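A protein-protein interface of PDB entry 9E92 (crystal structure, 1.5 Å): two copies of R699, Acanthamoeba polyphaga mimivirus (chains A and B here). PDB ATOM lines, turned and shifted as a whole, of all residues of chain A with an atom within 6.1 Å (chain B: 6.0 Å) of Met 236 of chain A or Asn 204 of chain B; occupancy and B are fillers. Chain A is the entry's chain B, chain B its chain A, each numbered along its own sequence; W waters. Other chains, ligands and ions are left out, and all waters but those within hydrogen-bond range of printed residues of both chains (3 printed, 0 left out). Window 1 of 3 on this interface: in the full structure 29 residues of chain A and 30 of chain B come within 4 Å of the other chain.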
ATOM      1  N   TYR A  34      -0.372 -21.191  26.988  1.00  0.00           N
ATOM      2  CA  TYR A  34       0.078 -22.580  27.009  1.00  0.00           C
ATOM      3  C   TYR A  34      -0.859 -23.430  27.884  1.00  0.00           C
ATOM      4  O   TYR A  34      -1.061 -24.576  27.547  1.00  0.00           O
ATOM      5  CB  TYR A  34       1.576 -22.693  27.419  1.00  0.00           C
ATOM      6  CG  TYR A  34       2.523 -22.497  26.230  1.00  0.00           C
ATOM      7  CD1 TYR A  34       2.745 -21.236  25.670  1.00  0.00           C
ATOM      8  CD2 TYR A  34       3.122 -23.591  25.629  1.00  0.00           C
ATOM      9  CE1 TYR A  34       3.583 -21.085  24.553  1.00  0.00           C
ATOM     10  CE2 TYR A  34       3.927 -23.450  24.507  1.00  0.00           C
ATOM     11  CZ  TYR A  34       4.186 -22.201  24.004  1.00  0.00           C
ATOM     12  OH  TYR A  34       4.966 -22.044  22.865  1.00  0.00           O
ATOM     13  N   ALA A  37      -3.796 -24.153  25.656  1.00  0.00           N
ATOM     14  CA  ALA A  37      -3.417 -25.078  24.592  1.00  0.00           C
ATOM     15  C   ALA A  37      -3.370 -26.524  25.068  1.00  0.00           C
ATOM     16  O   ALA A  37      -3.593 -27.436  24.262  1.00  0.00           O
ATOM     17  CB  ALA A  37      -2.075 -24.705  23.975  1.00  0.00           C
ATOM     18  N   HIS A  38      -3.032 -26.743  26.354  1.00  0.00           N
ATOM     19  CA  HIS A  38      -2.901 -28.065  26.922  1.00  0.00           C
ATOM     20  C   HIS A  38      -4.107 -28.488  27.774  1.00  0.00           C
ATOM     21  O   HIS A  38      -4.021 -29.492  28.473  1.00  0.00           O
ATOM     22  CB  HIS A  38      -1.557 -28.124  27.666  1.00  0.00           C
ATOM     23  CG  HIS A  38      -0.399 -28.045  26.726  1.00  0.00           C
ATOM     24  ND1 HIS A  38      -0.171 -29.103  25.860  1.00  0.00           N
ATOM     25  CD2 HIS A  38       0.518 -27.118  26.435  1.00  0.00           C
ATOM     26  CE1 HIS A  38       0.873 -28.803  25.082  1.00  0.00           C
ATOM     27  NE2 HIS A  38       1.293 -27.583  25.382  1.00  0.00           N
ATOM     28  N   ASN A 204       8.283 -31.104  19.916  1.00  0.00           N
ATOM     29  CA  ASN A 204       7.458 -30.102  20.595  1.00  0.00           C
ATOM     30  C   ASN A 204       7.552 -30.165  22.116  1.00  0.00           C
ATOM     31  O   ASN A 204       6.629 -29.763  22.800  1.00  0.00           O
ATOM     32  CB  ASN A 204       6.015 -30.076  20.113  1.00  0.00           C
ATOM     33  CG  ASN A 204       5.357 -28.732  20.358  1.00  0.00           C
ATOM     34  OD1 ASN A 204       5.965 -27.664  20.242  1.00  0.00           O
ATOM     35  ND2 ASN A 204       4.069 -28.786  20.668  1.00  0.00           N
ATOM     36  N   GLU A 232      11.184 -20.736  23.017  1.00  0.00           N
ATOM     37  CA  GLU A 232       9.783 -20.453  22.723  1.00  0.00           C
ATOM     38  C   GLU A 232       9.491 -20.419  21.223  1.00  0.00           C
ATOM     39  O   GLU A 232       8.445 -20.896  20.783  1.00  0.00           O
ATOM     40  CB  GLU A 232       9.445 -19.127  23.401  1.00  0.00           C
ATOM     41  CG  GLU A 232       8.026 -18.643  23.148  1.00  0.00           C
ATOM     42  CD  GLU A 232       7.695 -17.288  23.717  1.00  0.00           C
ATOM     43  OE1 GLU A 232       8.457 -16.769  24.519  1.00  0.00           O
ATOM     44  OE2 GLU A 232       6.642 -16.751  23.272  1.00  0.00           O
ATOM     45  N   TYR A 234      10.601 -22.188  18.942  1.00  0.00           N
ATOM     46  CA  TYR A 234      10.588 -23.527  18.369  1.00  0.00           C
ATOM     47  C   TYR A 234       9.440 -24.394  18.857  1.00  0.00           C
ATOM     48  O   TYR A 234       9.183 -25.467  18.239  1.00  0.00           O
ATOM     49  CB  TYR A 234      11.942 -24.206  18.640  1.00  0.00           C
ATOM     50  CG  TYR A 234      13.086 -23.489  17.969  1.00  0.00           C
ATOM     51  CD1 TYR A 234      13.736 -22.415  18.571  1.00  0.00           C
ATOM     52  CD2 TYR A 234      13.431 -23.786  16.668  1.00  0.00           C
ATOM     53  CE1 TYR A 234      14.767 -21.733  17.922  1.00  0.00           C
ATOM     54  CE2 TYR A 234      14.434 -23.096  16.003  1.00  0.00           C
ATOM     55  CZ  TYR A 234      15.119 -22.066  16.639  1.00  0.00           C
ATOM     56  OH  TYR A 234      16.051 -21.329  15.934  1.00  0.00           O
ATOM     57  N   PHE A 235       8.655 -23.916  19.837  1.00  0.00           N
ATOM     58  CA  PHE A 235       7.487 -24.633  20.322  1.00  0.00           C
ATOM     59  C   PHE A 235       6.242 -24.148  19.582  1.00  0.00           C
ATOM     60  O   PHE A 235       6.223 -23.053  19.009  1.00  0.00           O
ATOM     61  CB  PHE A 235       7.270 -24.406  21.819  1.00  0.00           C
ATOM     62  CG  PHE A 235       8.355 -24.934  22.752  1.00  0.00           C
ATOM     63  CD1 PHE A 235       8.841 -26.209  22.640  1.00  0.00           C
ATOM     64  CD2 PHE A 235       8.794 -24.125  23.807  1.00  0.00           C
ATOM     65  CE1 PHE A 235       9.832 -26.648  23.519  1.00  0.00           C
ATOM     66  CE2 PHE A 235       9.786 -24.561  24.647  1.00  0.00           C
ATOM     67  CZ  PHE A 235      10.303 -25.822  24.496  1.00  0.00           C
ATOM     68  N   MET A 236       5.205 -24.950  19.655  1.00  0.00           N
ATOM     69  CA  MET A 236       3.904 -24.542  19.130  1.00  0.00           C
ATOM     70  C   MET A 236       2.782 -24.889  20.102  1.00  0.00           C
ATOM     71  O   MET A 236       2.856 -25.854  20.866  1.00  0.00           O
ATOM     72  CB  MET A 236       3.620 -25.127  17.742  1.00  0.00           C
ATOM     73  CG  MET A 236       3.623 -26.603  17.713  1.00  0.00           C
ATOM     74  SD  MET A 236       3.464 -27.307  16.046  1.00  0.00           S
ATOM     75  CE  MET A 236       4.267 -28.846  16.449  1.00  0.00           C
ATOM     76  N   THR A 237       1.743 -24.037  20.077  1.00  0.00           N
ATOM     77  CA  THR A 237       0.547 -24.298  20.885  1.00  0.00           C
ATOM     78  C   THR A 237      -0.546 -25.005  20.080  1.00  0.00           C
ATOM     79  O   THR A 237      -1.541 -25.462  20.656  1.00  0.00           O
ATOM     80  CB  THR A 237       0.032 -22.984  21.474  1.00  0.00           C
ATOM     81  OG1 THR A 237      -0.165 -22.061  20.419  1.00  0.00           O
ATOM     82  CG2 THR A 237       0.968 -22.387  22.507  1.00  0.00           C
ATOM     83  N   GLU A 238      -0.417 -25.019  18.755  1.00  0.00           N
ATOM     84  CA  GLU A 238      -1.318 -25.724  17.854  1.00  0.00           C
ATOM     85  C   GLU A 238      -0.509 -26.059  16.606  1.00  0.00           C
ATOM     86  O   GLU A 238       0.476 -25.355  16.341  1.00  0.00           O
ATOM     87  CB  GLU A 238      -2.542 -24.861  17.519  1.00  0.00           C
ATOM     88  CG  GLU A 238      -2.234 -23.537  16.817  1.00  0.00           C
ATOM     89  CD  GLU A 238      -1.712 -22.376  17.675  1.00  0.00           C
ATOM     90  OE1 GLU A 238      -0.865 -21.582  17.183  1.00  0.00           O
ATOM     91  OE2 GLU A 238      -2.193 -22.205  18.832  1.00  0.00           O
ATOM     92  N   PRO A 239      -0.905 -27.052  15.787  1.00  0.00           N
ATOM     93  CA  PRO A 239      -0.168 -27.300  14.541  1.00  0.00           C
ATOM     94  C   PRO A 239      -0.133 -26.037  13.702  1.00  0.00           C
ATOM     95  O   PRO A 239      -1.109 -25.278  13.636  1.00  0.00           O
ATOM     96  CB  PRO A 239      -1.015 -28.368  13.843  1.00  0.00           C
ATOM     97  CG  PRO A 239      -1.626 -29.152  14.974  1.00  0.00           C
ATOM     98  CD  PRO A 239      -1.988 -28.030  15.999  1.00  0.00           C
ATOM     99  N   ILE A 240       0.962 -25.821  12.990  1.00  0.00           N
ATOM    100  CA  ILE A 240       1.066 -24.632  12.171  1.00  0.00           C
ATOM    101  C   ILE A 240       0.163 -24.751  10.933  1.00  0.00           C
ATOM    102  O   ILE A 240      -0.154 -25.844  10.456  1.00  0.00           O
ATOM    103  CB  ILE A 240       2.521 -24.378  11.799  1.00  0.00           C
ATOM    104  CG1 ILE A 240       2.919 -25.293  10.729  1.00  0.00           C
ATOM    105  CG2 ILE A 240       3.462 -24.469  13.008  1.00  0.00           C
ATOM    106  CD1 ILE A 240       2.882 -24.616   9.389  1.00  0.00           C
ATOM    107  N   HIS B  38      -3.447 -37.196   9.690  1.00  0.00           N
ATOM    108  CA  HIS B  38      -3.845 -35.896   9.177  1.00  0.00           C
ATOM    109  C   HIS B  38      -5.297 -35.915   8.639  1.00  0.00           C
ATOM    110  O   HIS B  38      -5.716 -34.964   7.993  1.00  0.00           O
ATOM    111  CB  HIS B  38      -2.806 -35.461   8.126  1.00  0.00           C
ATOM    112  CG  HIS B  38      -1.494 -35.192   8.761  1.00  0.00           C
ATOM    113  ND1 HIS B  38      -1.360 -34.092   9.585  1.00  0.00           N
ATOM    114  CD2 HIS B  38      -0.307 -35.804   8.719  1.00  0.00           C
ATOM    115  CE1 HIS B  38      -0.107 -34.099  10.088  1.00  0.00           C
ATOM    116  NE2 HIS B  38       0.534 -35.162   9.614  1.00  0.00           N
ATOM    117  N   LEU B  93       2.241 -34.285   5.505  1.00  0.00           N
ATOM    118  CA  LEU B  93       2.546 -33.580   6.757  1.00  0.00           C
ATOM    119  C   LEU B  93       1.426 -32.606   7.157  1.00  0.00           C
ATOM    120  O   LEU B  93       1.559 -31.912   8.167  1.00  0.00           O
ATOM    121  CB  LEU B  93       3.899 -32.872   6.694  1.00  0.00           C
ATOM    122  CG  LEU B  93       5.122 -33.783   6.523  1.00  0.00           C
ATOM    123  CD1 LEU B  93       6.405 -32.984   6.323  1.00  0.00           C
ATOM    124  CD2 LEU B  93       5.281 -34.765   7.712  1.00  0.00           C
ATOM    125  N   VAL B 201      13.703 -29.199   9.412  1.00  0.00           N
ATOM    126  CA  VAL B 201      12.603 -29.624  10.276  1.00  0.00           C
ATOM    127  C   VAL B 201      12.324 -28.512  11.280  1.00  0.00           C
ATOM    128  O   VAL B 201      13.210 -28.073  12.024  1.00  0.00           O
ATOM    129  CB  VAL B 201      12.846 -30.996  10.937  1.00  0.00           C
ATOM    130  CG1 VAL B 201      11.720 -31.361  11.863  1.00  0.00           C
ATOM    131  CG2 VAL B 201      13.002 -32.063   9.857  1.00  0.00           C
ATOM    132  N   HIS B 202      11.052 -28.107  11.347  1.00  0.00           N
ATOM    133  CA  HIS B 202      10.620 -27.029  12.240  1.00  0.00           C
ATOM    134  C   HIS B 202       9.135 -27.207  12.549  1.00  0.00           C
ATOM    135  O   HIS B 202       8.300 -27.372  11.622  1.00  0.00           O
ATOM    136  CB  HIS B 202      10.858 -25.689  11.544  1.00  0.00           C
ATOM    137  CG  HIS B 202      10.614 -24.493  12.419  1.00  0.00           C
ATOM    138  ND1 HIS B 202      11.350 -24.216  13.556  1.00  0.00           N
ATOM    139  CD2 HIS B 202       9.681 -23.501  12.322  1.00  0.00           C
ATOM    140  CE1 HIS B 202      10.898 -23.074  14.050  1.00  0.00           C
ATOM    141  NE2 HIS B 202       9.897 -22.625  13.357  1.00  0.00           N
ATOM    142  N   LYS B 203       8.778 -27.247  13.837  1.00  0.00           N
ATOM    143  CA  LYS B 203       7.379 -27.303  14.262  1.00  0.00           C
ATOM    144  C   LYS B 203       6.623 -28.440  13.536  1.00  0.00           C
ATOM    145  O   LYS B 203       5.505 -28.301  13.030  1.00  0.00           O
ATOM    146  CB  LYS B 203       6.730 -25.941  14.082  1.00  0.00           C
ATOM    147  CG  LYS B 203       7.291 -24.851  14.996  1.00  0.00           C
ATOM    148  CD  LYS B 203       6.584 -23.511  14.813  1.00  0.00           C
ATOM    149  CE  LYS B 203       7.186 -22.482  15.788  1.00  0.00           C
ATOM    150  NZ  LYS B 203       6.496 -21.199  15.655  1.00  0.00           N
ATOM    151  N   ASN B 204       7.267 -29.614  13.510  1.00  0.00           N
ATOM    152  CA  ASN B 204       6.686 -30.858  12.995  1.00  0.00           C
ATOM    153  C   ASN B 204       6.367 -30.773  11.516  1.00  0.00           C
ATOM    154  O   ASN B 204       5.505 -31.509  11.017  1.00  0.00           O
ATOM    155  CB  ASN B 204       5.443 -31.287  13.774  1.00  0.00           C
ATOM    156  CG  ASN B 204       5.156 -32.768  13.633  1.00  0.00           C
ATOM    157  OD1 ASN B 204       6.093 -33.589  13.641  1.00  0.00           O
ATOM    158  ND2 ASN B 204       3.887 -33.122  13.672  1.00  0.00           N
ATOM    159  N   ARG B 205       7.153 -29.960  10.800  1.00  0.00           N
ATOM    160  CA  ARG B 205       7.018 -29.750   9.375  1.00  0.00           C
ATOM    161  C   ARG B 205       8.379 -29.666   8.694  1.00  0.00           C
ATOM    162  O   ARG B 205       9.401 -29.440   9.348  1.00  0.00           O
ATOM    163  CB  ARG B 205       6.238 -28.461   9.065  1.00  0.00           C
ATOM    164  CG  ARG B 205       4.782 -28.413   9.552  1.00  0.00           C
ATOM    165  CD  ARG B 205       3.879 -29.422   8.805  1.00  0.00           C
ATOM    166  NE  ARG B 205       3.695 -29.058   7.405  1.00  0.00           N
ATOM    167  CZ  ARG B 205       2.687 -28.409   6.896  1.00  0.00           C
ATOM    168  NH1 ARG B 205       1.658 -27.996   7.634  1.00  0.00           N
ATOM    169  NH2 ARG B 205       2.617 -28.205   5.558  1.00  0.00           N
ATOM    170  N   ILE B 206       8.379 -29.807   7.364  1.00  0.00           N
ATOM    171  CA  ILE B 206       9.508 -29.346   6.543  1.00  0.00           C
ATOM    172  C   ILE B 206       9.261 -27.890   6.153  1.00  0.00           C
ATOM    173  O   ILE B 206       8.194 -27.547   5.608  1.00  0.00           O
ATOM    174  CB  ILE B 206       9.703 -30.201   5.279  1.00  0.00           C
ATOM    175  CG1 ILE B 206      10.136 -31.612   5.678  1.00  0.00           C
ATOM    176  CG2 ILE B 206      10.712 -29.524   4.348  1.00  0.00           C
ATOM    177  CD1 ILE B 206      10.294 -32.575   4.516  1.00  0.00           C
ATOM    178  N   TYR B 234      12.293 -37.357  13.665  1.00  0.00           N
ATOM    179  CA  TYR B 234      12.024 -36.058  14.293  1.00  0.00           C
ATOM    180  C   TYR B 234      10.576 -35.610  14.115  1.00  0.00           C
ATOM    181  O   TYR B 234      10.200 -34.591  14.694  1.00  0.00           O
ATOM    182  CB  TYR B 234      13.036 -35.011  13.770  1.00  0.00           C
ATOM    183  CG  TYR B 234      14.466 -35.392  14.125  1.00  0.00           C
ATOM    184  CD1 TYR B 234      15.268 -36.234  13.369  1.00  0.00           C
ATOM    185  CD2 TYR B 234      14.981 -34.952  15.346  1.00  0.00           C
ATOM    186  CE1 TYR B 234      16.534 -36.604  13.775  1.00  0.00           C
ATOM    187  CE2 TYR B 234      16.232 -35.362  15.799  1.00  0.00           C
ATOM    188  CZ  TYR B 234      17.030 -36.141  14.996  1.00  0.00           C
ATOM    189  OH  TYR B 234      18.286 -36.542  15.433  1.00  0.00           O
ATOM    190  N   PHE B 235       9.785 -36.330  13.276  1.00  0.00           N
ATOM    191  CA  PHE B 235       8.382 -36.036  13.100  1.00  0.00           C
ATOM    192  C   PHE B 235       7.544 -36.827  14.096  1.00  0.00           C
ATOM    193  O   PHE B 235       7.983 -37.864  14.621  1.00  0.00           O
ATOM    194  CB  PHE B 235       7.856 -36.341  11.680  1.00  0.00           C
ATOM    195  CG  PHE B 235       8.483 -35.578  10.528  1.00  0.00           C
ATOM    196  CD1 PHE B 235       8.679 -34.210  10.607  1.00  0.00           C
ATOM    197  CD2 PHE B 235       8.853 -36.229   9.358  1.00  0.00           C
ATOM    198  CE1 PHE B 235       9.255 -33.511   9.528  1.00  0.00           C
ATOM    199  CE2 PHE B 235       9.469 -35.539   8.321  1.00  0.00           C
ATOM    200  CZ  PHE B 235       9.649 -34.190   8.424  1.00  0.00           C
ATOM    201  N   MET B 236       6.297 -36.402  14.256  1.00  0.00           N
ATOM    202  CA  MET B 236       5.319 -37.154  15.050  1.00  0.00           C
ATOM    203  C   MET B 236       3.987 -37.185  14.296  1.00  0.00           C
ATOM    204  O   MET B 236       3.593 -36.222  13.627  1.00  0.00           O
ATOM    205  CB  MET B 236       5.238 -36.616  16.464  1.00  0.00           C
ATOM    206  CG  MET B 236       4.653 -35.233  16.540  1.00  0.00           C
ATOM    207  SD  MET B 236       4.855 -34.542  18.222  1.00  0.00           S
ATOM    208  CE  MET B 236       4.881 -32.832  17.684  1.00  0.00           C
ATOM    209  N   THR B 237       3.227 -38.278  14.554  1.00  0.00           N
ATOM    210  CA  THR B 237       1.871 -38.377  14.047  1.00  0.00           C
ATOM    211  C   THR B 237       0.851 -37.958  15.104  1.00  0.00           C
ATOM    212  O   THR B 237      -0.325 -37.806  14.775  1.00  0.00           O
ATOM    213  CB  THR B 237       1.585 -39.796  13.565  1.00  0.00           C
ATOM    214  OG1 THR B 237       1.873 -40.684  14.637  1.00  0.00           O
ATOM    215  CG2 THR B 237       2.447 -40.220  12.379  1.00  0.00           C
HETATM  216  O   HOH W   1       6.418 -20.282  18.995  1.00  0.00           O
HETATM  217  O   HOH W   2       2.733 -28.300  12.842  1.00  0.00           O
HETATM  218  O   HOH W   3       1.176 -28.244  10.554  1.00  0.00           O
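Printed residues of chain B within 4 Å of Asn 204 of chain A: Met 236.
Printed residues of chain B within 4 Å of Tyr 234 of chain A: His 202 (3.7 Å) and Lys 203 (3.8 Å).
Of the printed residues of chain B, Met 236 of chain A touches Lys 203 (3.7 Å) and Asn 204 (3.8 Å).
Of the printed residues of chain A, His 202 of chain B touches Tyr 234.
Of the printed residues of chain A, Lys 203 of chain B touches Tyr 234, Phe 235, Met 236 and Ile 240.
Of chain A, only Met 236 comes within 4 Å of Asn 204 of chain B.
Of the printed residues of chain A, Arg 205 of chain B touches Ile 240 (3.8 Å).
The nearest residue of chain B that does not touch Met 236 of chain A is Met 236 of chain B (4.2 Å).
The nearest printed residue of chain A that does not touch Asn 204 of chain B is Ile 240 of chain A (6.4 Å).
The nearest printed residue of chain B that does not touch Ile 240 of chain A is His 202 of chain B (5.8 Å).
Water W3 bridges the backbone carbonyl oxygen (O) of Ile 240 of chain A (2.7 Å) and the guanidinium group (NH1) of Arg 205 of chain B (3.0 Å).
Water W1 lies within hydrogen-bond range of O of Glu 232 of chain A, O of Phe 235 of chain A and NZ of Lys 203 of chain B.
Water W2 lies within hydrogen-bond range of O of Lys 203 of chain B, N of Ile 240 of chain A and SD of Met 236 of chain A.
Among the printed residues, merely in contact across the chains: Phe 235 of chain A with Lys 203 of chain B, Tyr 234 of chain A with His 202 of chain B, Ile 240 of chain A with Lys 203 of chain B, Tyr 234 of chain A with Lys 203 of chain B, Met 236 of chain A with Asn 204 of chain B, Ile 240 of chain A with Arg 205 of chain B and Asn 204 of chain A with Met 236 of chain B.
The backbone carbonyl oxygen (O) of Lys 203 of chain B lies close to the side-chain sulfur (SD) of Met 236 of chain A (3.8 Å).
Of the 12 printed residues of chain A, 5 touch a printed residue of chain B.
Printed residues of chain A that touch a printed residue of chain B: Asn 204, Tyr 234, Phe 235, Met 236 and Ile 240.
Hydrophobic or aromatic side chains of chain A that line the printed part of chain B: Tyr 234, Met 236 and Ile 240.
Printed residues of chain B that touch a printed residue of chain A: His 202, Lys 203, Asn 204, Arg 205 and Met 236.
Asn 204 of chain A touches Met 236 of chain B, and with the chains exchanged Met 236 of chain A touches Asn 204 of chain B.
OD1 of Asn 204 of chain B sits at hydrogen-bond distance from N of Met 236 of chain B, at 2.9 Å.
The side-chain amide oxygen (OD1) of Asn 204 of chain A sits at hydrogen-bond distance from the backbone NH (N) of Met 236 of chain A, at 2.9 Å.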
